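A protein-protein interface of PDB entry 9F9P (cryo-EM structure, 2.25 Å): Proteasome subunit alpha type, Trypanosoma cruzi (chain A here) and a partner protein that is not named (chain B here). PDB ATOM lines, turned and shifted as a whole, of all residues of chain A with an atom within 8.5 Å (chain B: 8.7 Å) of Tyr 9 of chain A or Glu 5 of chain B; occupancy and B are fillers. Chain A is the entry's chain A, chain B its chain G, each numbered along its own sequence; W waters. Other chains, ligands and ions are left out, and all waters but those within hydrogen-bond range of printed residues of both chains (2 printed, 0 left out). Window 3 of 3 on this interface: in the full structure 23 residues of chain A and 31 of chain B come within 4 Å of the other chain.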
ATOM      1  N   PHE A   6      22.426  11.749  -7.820  1.00  0.00           N
ATOM      2  CA  PHE A   6      22.531  13.239  -7.818  1.00  0.00           C
ATOM      3  C   PHE A   6      21.328  13.824  -8.567  1.00  0.00           C
ATOM      4  O   PHE A   6      20.590  14.650  -8.044  1.00  0.00           O
ATOM      5  CB  PHE A   6      23.889  13.615  -8.403  1.00  0.00           C
ATOM      6  CG  PHE A   6      24.484  14.923  -7.955  1.00  0.00           C
ATOM      7  CD1 PHE A   6      25.532  14.943  -7.032  1.00  0.00           C
ATOM      8  CD2 PHE A   6      24.106  16.116  -8.557  1.00  0.00           C
ATOM      9  CE1 PHE A   6      26.154  16.134  -6.679  1.00  0.00           C
ATOM     10  CE2 PHE A   6      24.728  17.309  -8.203  1.00  0.00           C
ATOM     11  CZ  PHE A   6      25.748  17.316  -7.265  1.00  0.00           C
ATOM     12  N   ASP A   7      21.123  13.337  -9.784  1.00  0.00           N
ATOM     13  CA  ASP A   7      19.856  13.432 -10.482  1.00  0.00           C
ATOM     14  C   ASP A   7      18.715  12.722  -9.728  1.00  0.00           C
ATOM     15  O   ASP A   7      17.542  13.032  -9.942  1.00  0.00           O
ATOM     16  CB  ASP A   7      19.973  12.855 -11.903  1.00  0.00           C
ATOM     17  CG  ASP A   7      20.587  11.468 -12.006  1.00  0.00           C
ATOM     18  OD1 ASP A   7      21.302  11.060 -11.069  1.00  0.00           O
ATOM     19  OD2 ASP A   7      20.345  10.803 -13.019  1.00  0.00           O
ATOM     20  N   LYS A   8      19.044  11.789  -8.830  1.00  0.00           N
ATOM     21  CA  LYS A   8      18.042  11.156  -7.990  1.00  0.00           C
ATOM     22  C   LYS A   8      17.572  12.047  -6.851  1.00  0.00           C
ATOM     23  O   LYS A   8      16.480  11.804  -6.356  1.00  0.00           O
ATOM     24  CB  LYS A   8      18.540   9.817  -7.467  1.00  0.00           C
ATOM     25  CG  LYS A   8      18.978   8.911  -8.592  1.00  0.00           C
ATOM     26  CD  LYS A   8      18.237   7.610  -8.693  1.00  0.00           C
ATOM     27  CE  LYS A   8      18.601   6.876  -9.972  1.00  0.00           C
ATOM     28  NZ  LYS A   8      20.034   6.476  -9.978  1.00  0.00           N
ATOM     29  N   TYR A   9      18.322  13.086  -6.481  1.00  0.00           N
ATOM     30  CA  TYR A   9      18.039  13.809  -5.247  1.00  0.00           C
ATOM     31  C   TYR A   9      17.536  15.222  -5.513  1.00  0.00           C
ATOM     32  O   TYR A   9      16.752  15.717  -4.723  1.00  0.00           O
ATOM     33  CB  TYR A   9      19.257  13.792  -4.307  1.00  0.00           C
ATOM     34  CG  TYR A   9      19.769  12.393  -4.055  1.00  0.00           C
ATOM     35  CD1 TYR A   9      18.883  11.382  -3.694  1.00  0.00           C
ATOM     36  CD2 TYR A   9      21.105  12.046  -4.244  1.00  0.00           C
ATOM     37  CE1 TYR A   9      19.300  10.076  -3.524  1.00  0.00           C
ATOM     38  CE2 TYR A   9      21.549  10.745  -4.016  1.00  0.00           C
ATOM     39  CZ  TYR A   9      20.638   9.754  -3.665  1.00  0.00           C
ATOM     40  OH  TYR A   9      20.982   8.431  -3.475  1.00  0.00           O
ATOM     41  N   ILE A  10      17.939  15.869  -6.610  1.00  0.00           N
ATOM     42  CA  ILE A  10      17.430  17.199  -6.912  1.00  0.00           C
ATOM     43  C   ILE A  10      16.838  17.243  -8.315  1.00  0.00           C
ATOM     44  O   ILE A  10      16.954  16.284  -9.068  1.00  0.00           O
ATOM     45  CB  ILE A  10      18.535  18.254  -6.719  1.00  0.00           C
ATOM     46  CG1 ILE A  10      19.844  17.834  -7.376  1.00  0.00           C
ATOM     47  CG2 ILE A  10      18.738  18.562  -5.243  1.00  0.00           C
ATOM     48  CD1 ILE A  10      20.810  18.973  -7.529  1.00  0.00           C
ATOM     49  N   THR A  11      16.191  18.366  -8.638  1.00  0.00           N
ATOM     50  CA  THR A  11      15.657  18.609  -9.970  1.00  0.00           C
ATOM     51  C   THR A  11      16.770  19.067 -10.917  1.00  0.00           C
ATOM     52  O   THR A  11      17.042  20.246 -11.027  1.00  0.00           O
ATOM     53  CB  THR A  11      14.483  19.614  -9.954  1.00  0.00           C
ATOM     54  OG1 THR A  11      14.814  20.820  -9.241  1.00  0.00           O
ATOM     55  CG2 THR A  11      13.208  18.990  -9.403  1.00  0.00           C
ATOM     56  N   VAL A  12      17.463  18.096 -11.513  1.00  0.00           N
ATOM     57  CA  VAL A  12      18.276  18.268 -12.695  1.00  0.00           C
ATOM     58  C   VAL A  12      17.929  17.113 -13.607  1.00  0.00           C
ATOM     59  O   VAL A  12      17.387  16.138 -13.132  1.00  0.00           O
ATOM     60  CB  VAL A  12      19.789  18.264 -12.376  1.00  0.00           C
ATOM     61  CG1 VAL A  12      20.173  19.437 -11.500  1.00  0.00           C
ATOM     62  CG2 VAL A  12      20.252  16.962 -11.753  1.00  0.00           C
ATOM     63  N   LEU A  19      13.251  13.504 -15.256  1.00  0.00           N
ATOM     64  CA  LEU A  19      13.360  14.076 -13.921  1.00  0.00           C
ATOM     65  C   LEU A  19      12.847  13.094 -12.869  1.00  0.00           C
ATOM     66  O   LEU A  19      11.651  12.860 -12.755  1.00  0.00           O
ATOM     67  CB  LEU A  19      12.546  15.372 -13.877  1.00  0.00           C
ATOM     68  CG  LEU A  19      12.915  16.443 -14.918  1.00  0.00           C
ATOM     69  CD1 LEU A  19      11.755  17.427 -15.161  1.00  0.00           C
ATOM     70  CD2 LEU A  19      14.130  17.239 -14.459  1.00  0.00           C
ATOM     71  N   TYR A  20      13.750  12.550 -12.050  1.00  0.00           N
ATOM     72  CA  TYR A  20      13.420  11.458 -11.151  1.00  0.00           C
ATOM     73  C   TYR A  20      12.599  11.949  -9.970  1.00  0.00           C
ATOM     74  O   TYR A  20      11.686  11.264  -9.551  1.00  0.00           O
ATOM     75  CB  TYR A  20      14.679  10.745 -10.680  1.00  0.00           C
ATOM     76  CG  TYR A  20      15.302   9.817 -11.690  1.00  0.00           C
ATOM     77  CD1 TYR A  20      14.623   8.712 -12.182  1.00  0.00           C
ATOM     78  CD2 TYR A  20      16.609  10.003 -12.111  1.00  0.00           C
ATOM     79  CE1 TYR A  20      15.205   7.852 -13.100  1.00  0.00           C
ATOM     80  CE2 TYR A  20      17.207   9.152 -13.026  1.00  0.00           C
ATOM     81  CZ  TYR A  20      16.499   8.082 -13.531  1.00  0.00           C
ATOM     82  OH  TYR A  20      17.132   7.262 -14.424  1.00  0.00           O
ATOM     83  N   GLN A  21      12.852  13.137  -9.441  1.00  0.00           N
ATOM     84  CA  GLN A  21      12.008  13.558  -8.344  1.00  0.00           C
ATOM     85  C   GLN A  21      10.552  13.671  -8.823  1.00  0.00           C
ATOM     86  O   GLN A  21       9.644  13.484  -8.018  1.00  0.00           O
ATOM     87  CB  GLN A  21      12.504  14.855  -7.685  1.00  0.00           C
ATOM     88  CG  GLN A  21      13.632  14.663  -6.669  1.00  0.00           C
ATOM     89  CD  GLN A  21      13.153  13.880  -5.467  1.00  0.00           C
ATOM     90  OE1 GLN A  21      12.174  14.255  -4.820  1.00  0.00           O
ATOM     91  NE2 GLN A  21      13.849  12.805  -5.151  1.00  0.00           N
ATOM     92  N   TYR A  24       8.971  10.107  -8.752  1.00  0.00           N
ATOM     93  CA  TYR A  24       8.832   9.572  -7.415  1.00  0.00           C
ATOM     94  C   TYR A  24       7.675  10.225  -6.673  1.00  0.00           C
ATOM     95  O   TYR A  24       6.974   9.574  -5.916  1.00  0.00           O
ATOM     96  CB  TYR A  24      10.106   9.838  -6.616  1.00  0.00           C
ATOM     97  CG  TYR A  24      11.351   9.094  -7.052  1.00  0.00           C
ATOM     98  CD1 TYR A  24      11.323   8.077  -7.999  1.00  0.00           C
ATOM     99  CD2 TYR A  24      12.589   9.443  -6.504  1.00  0.00           C
ATOM    100  CE1 TYR A  24      12.488   7.434  -8.401  1.00  0.00           C
ATOM    101  CE2 TYR A  24      13.757   8.784  -6.871  1.00  0.00           C
ATOM    102  CZ  TYR A  24      13.700   7.762  -7.809  1.00  0.00           C
ATOM    103  OH  TYR A  24      14.869   7.139  -8.150  1.00  0.00           O
ATOM    104  N   ALA A 126      15.634  24.403  -7.346  1.00  0.00           N
ATOM    105  CA  ALA A 126      16.064  23.460  -6.316  1.00  0.00           C
ATOM    106  C   ALA A 126      15.638  23.872  -4.898  1.00  0.00           C
ATOM    107  O   ALA A 126      15.492  25.040  -4.604  1.00  0.00           O
ATOM    108  CB  ALA A 126      17.560  23.284  -6.355  1.00  0.00           C
ATOM    109  N   GLY A 127      15.403  22.878  -4.030  1.00  0.00           N
ATOM    110  CA  GLY A 127      15.309  23.112  -2.591  1.00  0.00           C
ATOM    111  C   GLY A 127      13.916  23.009  -1.947  1.00  0.00           C
ATOM    112  O   GLY A 127      13.837  22.940  -0.725  1.00  0.00           O
ATOM    113  N   LEU A 128      12.824  23.021  -2.708  1.00  0.00           N
ATOM    114  CA  LEU A 128      11.506  22.766  -2.129  1.00  0.00           C
ATOM    115  C   LEU A 128      10.961  21.470  -2.716  1.00  0.00           C
ATOM    116  O   LEU A 128      11.086  21.230  -3.893  1.00  0.00           O
ATOM    117  CB  LEU A 128      10.597  23.971  -2.403  1.00  0.00           C
ATOM    118  CG  LEU A 128      10.916  25.268  -1.646  1.00  0.00           C
ATOM    119  CD1 LEU A 128      10.124  26.447  -2.184  1.00  0.00           C
ATOM    120  CD2 LEU A 128      10.588  25.166  -0.135  1.00  0.00           C
ATOM    121  N   ARG A 129      10.421  20.601  -1.876  1.00  0.00           N
ATOM    122  CA  ARG A 129       9.900  19.311  -2.284  1.00  0.00           C
ATOM    123  C   ARG A 129       8.668  19.481  -3.167  1.00  0.00           C
ATOM    124  O   ARG A 129       7.863  20.369  -2.938  1.00  0.00           O
ATOM    125  CB  ARG A 129       9.586  18.543  -1.008  1.00  0.00           C
ATOM    126  CG  ARG A 129       9.099  17.125  -1.226  1.00  0.00           C
ATOM    127  CD  ARG A 129       9.065  16.257   0.000  1.00  0.00           C
ATOM    128  NE  ARG A 129       8.219  16.781   1.038  1.00  0.00           N
ATOM    129  CZ  ARG A 129       6.903  16.787   1.009  1.00  0.00           C
ATOM    130  NH1 ARG A 129       6.216  16.334  -0.040  1.00  0.00           N
ATOM    131  NH2 ARG A 129       6.244  17.256   2.055  1.00  0.00           N
ATOM    132  N   THR B   4      21.412   5.299  -0.127  1.00  0.00           N
ATOM    133  CA  THR B   4      20.767   5.759   1.138  1.00  0.00           C
ATOM    134  C   THR B   4      21.132   7.218   1.422  1.00  0.00           C
ATOM    135  O   THR B   4      21.368   7.582   2.577  1.00  0.00           O
ATOM    136  CB  THR B   4      21.150   4.890   2.354  1.00  0.00           C
ATOM    137  OG1 THR B   4      22.565   4.956   2.548  1.00  0.00           O
ATOM    138  CG2 THR B   4      20.720   3.442   2.238  1.00  0.00           C
ATOM    139  N   GLU B   5      21.191   8.043   0.368  1.00  0.00           N
ATOM    140  CA  GLU B   5      21.403   9.475   0.528  1.00  0.00           C
ATOM    141  C   GLU B   5      20.053  10.174   0.591  1.00  0.00           C
ATOM    142  O   GLU B   5      19.968  11.350   0.932  1.00  0.00           O
ATOM    143  CB  GLU B   5      22.233  10.065  -0.614  1.00  0.00           C
ATOM    144  CG  GLU B   5      23.690  10.319  -0.256  1.00  0.00           C
ATOM    145  CD  GLU B   5      24.429  11.222  -1.237  1.00  0.00           C
ATOM    146  OE1 GLU B   5      23.973  12.371  -1.457  1.00  0.00           O
ATOM    147  OE2 GLU B   5      25.467  10.781  -1.777  1.00  0.00           O
ATOM    148  N   HIS B   6      19.002   9.417   0.296  1.00  0.00           N
ATOM    149  CA  HIS B   6      17.666   9.961   0.158  1.00  0.00           C
ATOM    150  C   HIS B   6      17.046  10.312   1.505  1.00  0.00           C
ATOM    151  O   HIS B   6      15.932  10.834   1.514  1.00  0.00           O
ATOM    152  CB  HIS B   6      16.751   8.987  -0.594  1.00  0.00           C
ATOM    153  CG  HIS B   6      16.537   7.668   0.060  1.00  0.00           C
ATOM    154  ND1 HIS B   6      17.329   6.586  -0.242  1.00  0.00           N
ATOM    155  CD2 HIS B   6      15.670   7.248   0.995  1.00  0.00           C
ATOM    156  CE1 HIS B   6      16.942   5.543   0.481  1.00  0.00           C
ATOM    157  NE2 HIS B   6      15.928   5.921   1.233  1.00  0.00           N
ATOM    158  N   ASP B   7      17.742  10.053   2.627  1.00  0.00           N
ATOM    159  CA  ASP B   7      17.114  10.218   3.928  1.00  0.00           C
ATOM    160  C   ASP B   7      17.807  11.291   4.750  1.00  0.00           C
ATOM    161  O   ASP B   7      17.599  11.372   5.950  1.00  0.00           O
ATOM    162  CB  ASP B   7      17.051   8.885   4.651  1.00  0.00           C
ATOM    163  CG  ASP B   7      18.394   8.465   5.184  1.00  0.00           C
ATOM    164  OD1 ASP B   7      18.410   7.502   6.009  1.00  0.00           O
ATOM    165  OD2 ASP B   7      19.399   9.153   4.825  1.00  0.00           O
ATOM    166  N   GLN B   8      18.530  12.179   4.081  1.00  0.00           N
ATOM    167  CA  GLN B   8      19.309  13.198   4.743  1.00  0.00           C
ATOM    168  C   GLN B   8      18.545  14.515   4.830  1.00  0.00           C
ATOM    169  O   GLN B   8      18.916  15.376   5.624  1.00  0.00           O
ATOM    170  CB  GLN B   8      20.587  13.445   3.948  1.00  0.00           C
ATOM    171  CG  GLN B   8      21.614  12.313   4.047  1.00  0.00           C
ATOM    172  CD  GLN B   8      22.337  12.346   5.377  1.00  0.00           C
ATOM    173  OE1 GLN B   8      23.042  13.302   5.692  1.00  0.00           O
ATOM    174  NE2 GLN B   8      22.123  11.328   6.187  1.00  0.00           N
ATOM    175  N   SER B   9      17.518  14.731   3.995  1.00  0.00           N
ATOM    176  CA  SER B   9      16.764  15.966   4.131  1.00  0.00           C
ATOM    177  C   SER B   9      15.307  15.744   3.821  1.00  0.00           C
ATOM    178  O   SER B   9      14.939  14.795   3.139  1.00  0.00           O
ATOM    179  CB  SER B   9      17.333  17.087   3.301  1.00  0.00           C
ATOM    180  OG  SER B   9      17.323  16.767   1.924  1.00  0.00           O
ATOM    181  N   THR B  10      14.489  16.653   4.350  1.00  0.00           N
ATOM    182  CA  THR B  10      13.061  16.510   4.191  1.00  0.00           C
ATOM    183  C   THR B  10      12.582  16.953   2.797  1.00  0.00           C
ATOM    184  O   THR B  10      11.428  16.716   2.476  1.00  0.00           O
ATOM    185  CB  THR B  10      12.287  17.174   5.328  1.00  0.00           C
ATOM    186  OG1 THR B  10      10.949  16.653   5.258  1.00  0.00           O
ATOM    187  CG2 THR B  10      12.267  18.680   5.230  1.00  0.00           C
ATOM    188  N   ASP B  11      13.452  17.485   1.937  1.00  0.00           N
ATOM    189  CA  ASP B  11      13.017  17.997   0.647  1.00  0.00           C
ATOM    190  C   ASP B  11      13.099  16.970  -0.484  1.00  0.00           C
ATOM    191  O   ASP B  11      12.836  17.345  -1.615  1.00  0.00           O
ATOM    192  CB  ASP B  11      13.766  19.272   0.260  1.00  0.00           C
ATOM    193  CG  ASP B  11      15.256  19.081   0.039  1.00  0.00           C
ATOM    194  OD1 ASP B  11      15.792  19.715  -0.901  1.00  0.00           O
ATOM    195  OD2 ASP B  11      15.878  18.278   0.808  1.00  0.00           O
ATOM    196  N   ILE B  12      13.312  15.688  -0.180  1.00  0.00           N
ATOM    197  CA  ILE B  12      13.568  14.640  -1.161  1.00  0.00           C
ATOM    198  C   ILE B  12      12.606  13.460  -0.975  1.00  0.00           C
ATOM    199  O   ILE B  12      12.603  12.848   0.076  1.00  0.00           O
ATOM    200  CB  ILE B  12      14.998  14.139  -0.918  1.00  0.00           C
ATOM    201  CG1 ILE B  12      16.039  15.227  -1.148  1.00  0.00           C
ATOM    202  CG2 ILE B  12      15.342  12.922  -1.744  1.00  0.00           C
ATOM    203  CD1 ILE B  12      17.386  14.834  -0.596  1.00  0.00           C
ATOM    204  N   PHE B  13      11.892  13.055  -2.022  1.00  0.00           N
ATOM    205  CA  PHE B  13      11.240  11.762  -2.042  1.00  0.00           C
ATOM    206  C   PHE B  13      12.252  10.641  -2.248  1.00  0.00           C
ATOM    207  O   PHE B  13      13.267  10.824  -2.908  1.00  0.00           O
ATOM    208  CB  PHE B  13      10.206  11.637  -3.169  1.00  0.00           C
ATOM    209  CG  PHE B  13       8.929  12.402  -2.949  1.00  0.00           C
ATOM    210  CD1 PHE B  13       8.014  11.998  -2.005  1.00  0.00           C
ATOM    211  CD2 PHE B  13       8.690  13.593  -3.628  1.00  0.00           C
ATOM    212  CE1 PHE B  13       6.872  12.730  -1.755  1.00  0.00           C
ATOM    213  CE2 PHE B  13       7.560  14.350  -3.363  1.00  0.00           C
ATOM    214  CZ  PHE B  13       6.634  13.893  -2.444  1.00  0.00           C
ATOM    215  N   SER B  14      11.952   9.480  -1.670  1.00  0.00           N
ATOM    216  CA  SER B  14      12.575   8.205  -1.998  1.00  0.00           C
ATOM    217  C   SER B  14      11.901   7.618  -3.234  1.00  0.00           C
ATOM    218  O   SER B  14      10.780   8.015  -3.550  1.00  0.00           O
ATOM    219  CB  SER B  14      12.381   7.254  -0.823  1.00  0.00           C
ATOM    220  OG  SER B  14      11.127   6.577  -0.878  1.00  0.00           O
ATOM    221  N   ALA B  15      12.516   6.598  -3.837  1.00  0.00           N
ATOM    222  CA  ALA B  15      11.980   5.900  -5.006  1.00  0.00           C
ATOM    223  C   ALA B  15      10.576   5.327  -4.815  1.00  0.00           C
ATOM    224  O   ALA B  15       9.869   5.083  -5.782  1.00  0.00           O
ATOM    225  CB  ALA B  15      12.885   4.763  -5.397  1.00  0.00           C
ATOM    226  N   PHE B  20      11.534  10.077   4.246  1.00  0.00           N
ATOM    227  CA  PHE B  20      12.067   9.393   5.426  1.00  0.00           C
ATOM    228  C   PHE B  20      12.312  10.319   6.617  1.00  0.00           C
ATOM    229  O   PHE B  20      12.035   9.935   7.731  1.00  0.00           O
ATOM    230  CB  PHE B  20      13.340   8.639   5.086  1.00  0.00           C
ATOM    231  CG  PHE B  20      13.127   7.295   4.450  1.00  0.00           C
ATOM    232  CD1 PHE B  20      13.711   6.164   4.964  1.00  0.00           C
ATOM    233  CD2 PHE B  20      12.363   7.144   3.316  1.00  0.00           C
ATOM    234  CE1 PHE B  20      13.557   4.934   4.344  1.00  0.00           C
ATOM    235  CE2 PHE B  20      12.183   5.900   2.715  1.00  0.00           C
ATOM    236  CZ  PHE B  20      12.778   4.798   3.224  1.00  0.00           C
ATOM    237  N   GLN B  21      12.796  11.543   6.434  1.00  0.00           N
ATOM    238  CA  GLN B  21      12.978  12.410   7.587  1.00  0.00           C
ATOM    239  C   GLN B  21      11.687  12.579   8.379  1.00  0.00           C
ATOM    240  O   GLN B  21      11.730  12.799   9.572  1.00  0.00           O
ATOM    241  CB  GLN B  21      13.495  13.798   7.175  1.00  0.00           C
ATOM    242  CG  GLN B  21      15.000  13.866   6.957  1.00  0.00           C
ATOM    243  CD  GLN B  21      15.790  13.671   8.231  1.00  0.00           C
ATOM    244  OE1 GLN B  21      15.740  14.497   9.141  1.00  0.00           O
ATOM    245  NE2 GLN B  21      16.493  12.550   8.305  1.00  0.00           N
ATOM    246  N   TYR B  24      11.172   9.416  10.555  1.00  0.00           N
ATOM    247  CA  TYR B  24      12.092   9.409  11.673  1.00  0.00           C
ATOM    248  C   TYR B  24      11.604  10.324  12.794  1.00  0.00           C
ATOM    249  O   TYR B  24      11.791  10.013  13.962  1.00  0.00           O
ATOM    250  CB  TYR B  24      13.490   9.853  11.219  1.00  0.00           C
ATOM    251  CG  TYR B  24      14.195   8.931  10.244  1.00  0.00           C
ATOM    252  CD1 TYR B  24      13.722   7.674   9.925  1.00  0.00           C
ATOM    253  CD2 TYR B  24      15.345   9.350   9.591  1.00  0.00           C
ATOM    254  CE1 TYR B  24      14.391   6.853   9.022  1.00  0.00           C
ATOM    255  CE2 TYR B  24      15.995   8.558   8.651  1.00  0.00           C
ATOM    256  CZ  TYR B  24      15.531   7.296   8.376  1.00  0.00           C
ATOM    257  OH  TYR B  24      16.247   6.526   7.468  1.00  0.00           O
HETATM  258  O   HOH W   1      15.858   9.902  -3.921  1.00  0.00           O
HETATM  259  O   HOH W   2      11.182  16.805  -4.385  1.00  0.00           O
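The side-chain amide nitrogen of Gln 21 of chain A lies within hydrogen-bond range of the backbone carbonyl oxygen of Phe 13 of chain B.
The side-chain amide nitrogen (NE2) of Gln 21 of chain A is in hydrogen-bond range of the backbone carbonyl oxygen (O) of Lys 8 of chain A (3.1 Å).
Among the printed residues, merely in contact across the chains: Arg 129 of chain A with Phe 13 of chain B (3.5 Å), Arg 129 of chain A with Thr 10 of chain B (3.5 Å), Tyr 9 of chain A with Glu 5 of chain B (3.5 Å), Arg 129 of chain A with Asp 11 of chain B (3.5 Å), Tyr 24 of chain A with Ser 14 of chain B (3.6 Å), Tyr 9 of chain A with Ile 12 of chain B (3.7 Å), Gln 21 of chain A with Ile 12 of chain B (3.7 Å), Tyr 24 of chain A with Ala 15 of chain B (3.8 Å), Gly 127 of chain A with Asp 11 of chain B (3.8 Å), Tyr 9 of chain A with His 6 of chain B (3.9 Å) and Tyr 24 of chain A with Phe 13 of chain B (3.9 Å).
Tyr 9 of chain A touches three residues of chain B. Of the printed residues of chain B, Gly 127 of chain A touches Asp 11 (3.8 Å). Glu 5 of chain B touches one residue of chain A. Of the printed residues of chain A, Thr 10 of chain B touches Arg 129. Of the printed residues of chain A, Asp 11 of chain B touches Gly 127 and Arg 129. Of the printed residues of chain A, Ser 14 of chain B touches Tyr 24. The nearest residue of chain B that does not touch Tyr 9 of chain A is Thr 4 of chain B (4.6 Å). The nearest residue of chain A that does not touch Glu 5 of chain B is Phe 6 of chain A (6.3 Å). The nearest printed residue of chain A that does not touch Phe 13 of chain B is Lys 8 of chain A (4.8 Å).
Among the printed residues, 12 pairs touch across the chains. Among the printed residues, no Asp or Glu carboxylate lies within 4 Å of a Lys or Arg side-chain nitrogen of the other chain.
Water W2 bridges the side-chain amide oxygen (OE1) of Gln 21 of chain A and the backbone carbonyl oxygen (O) of Asp 11 of chain B. Water W1 bridges the backbone carbonyl oxygen of Phe 13 of chain B and the backbone carbonyl oxygen of Lys 8 of chain A.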
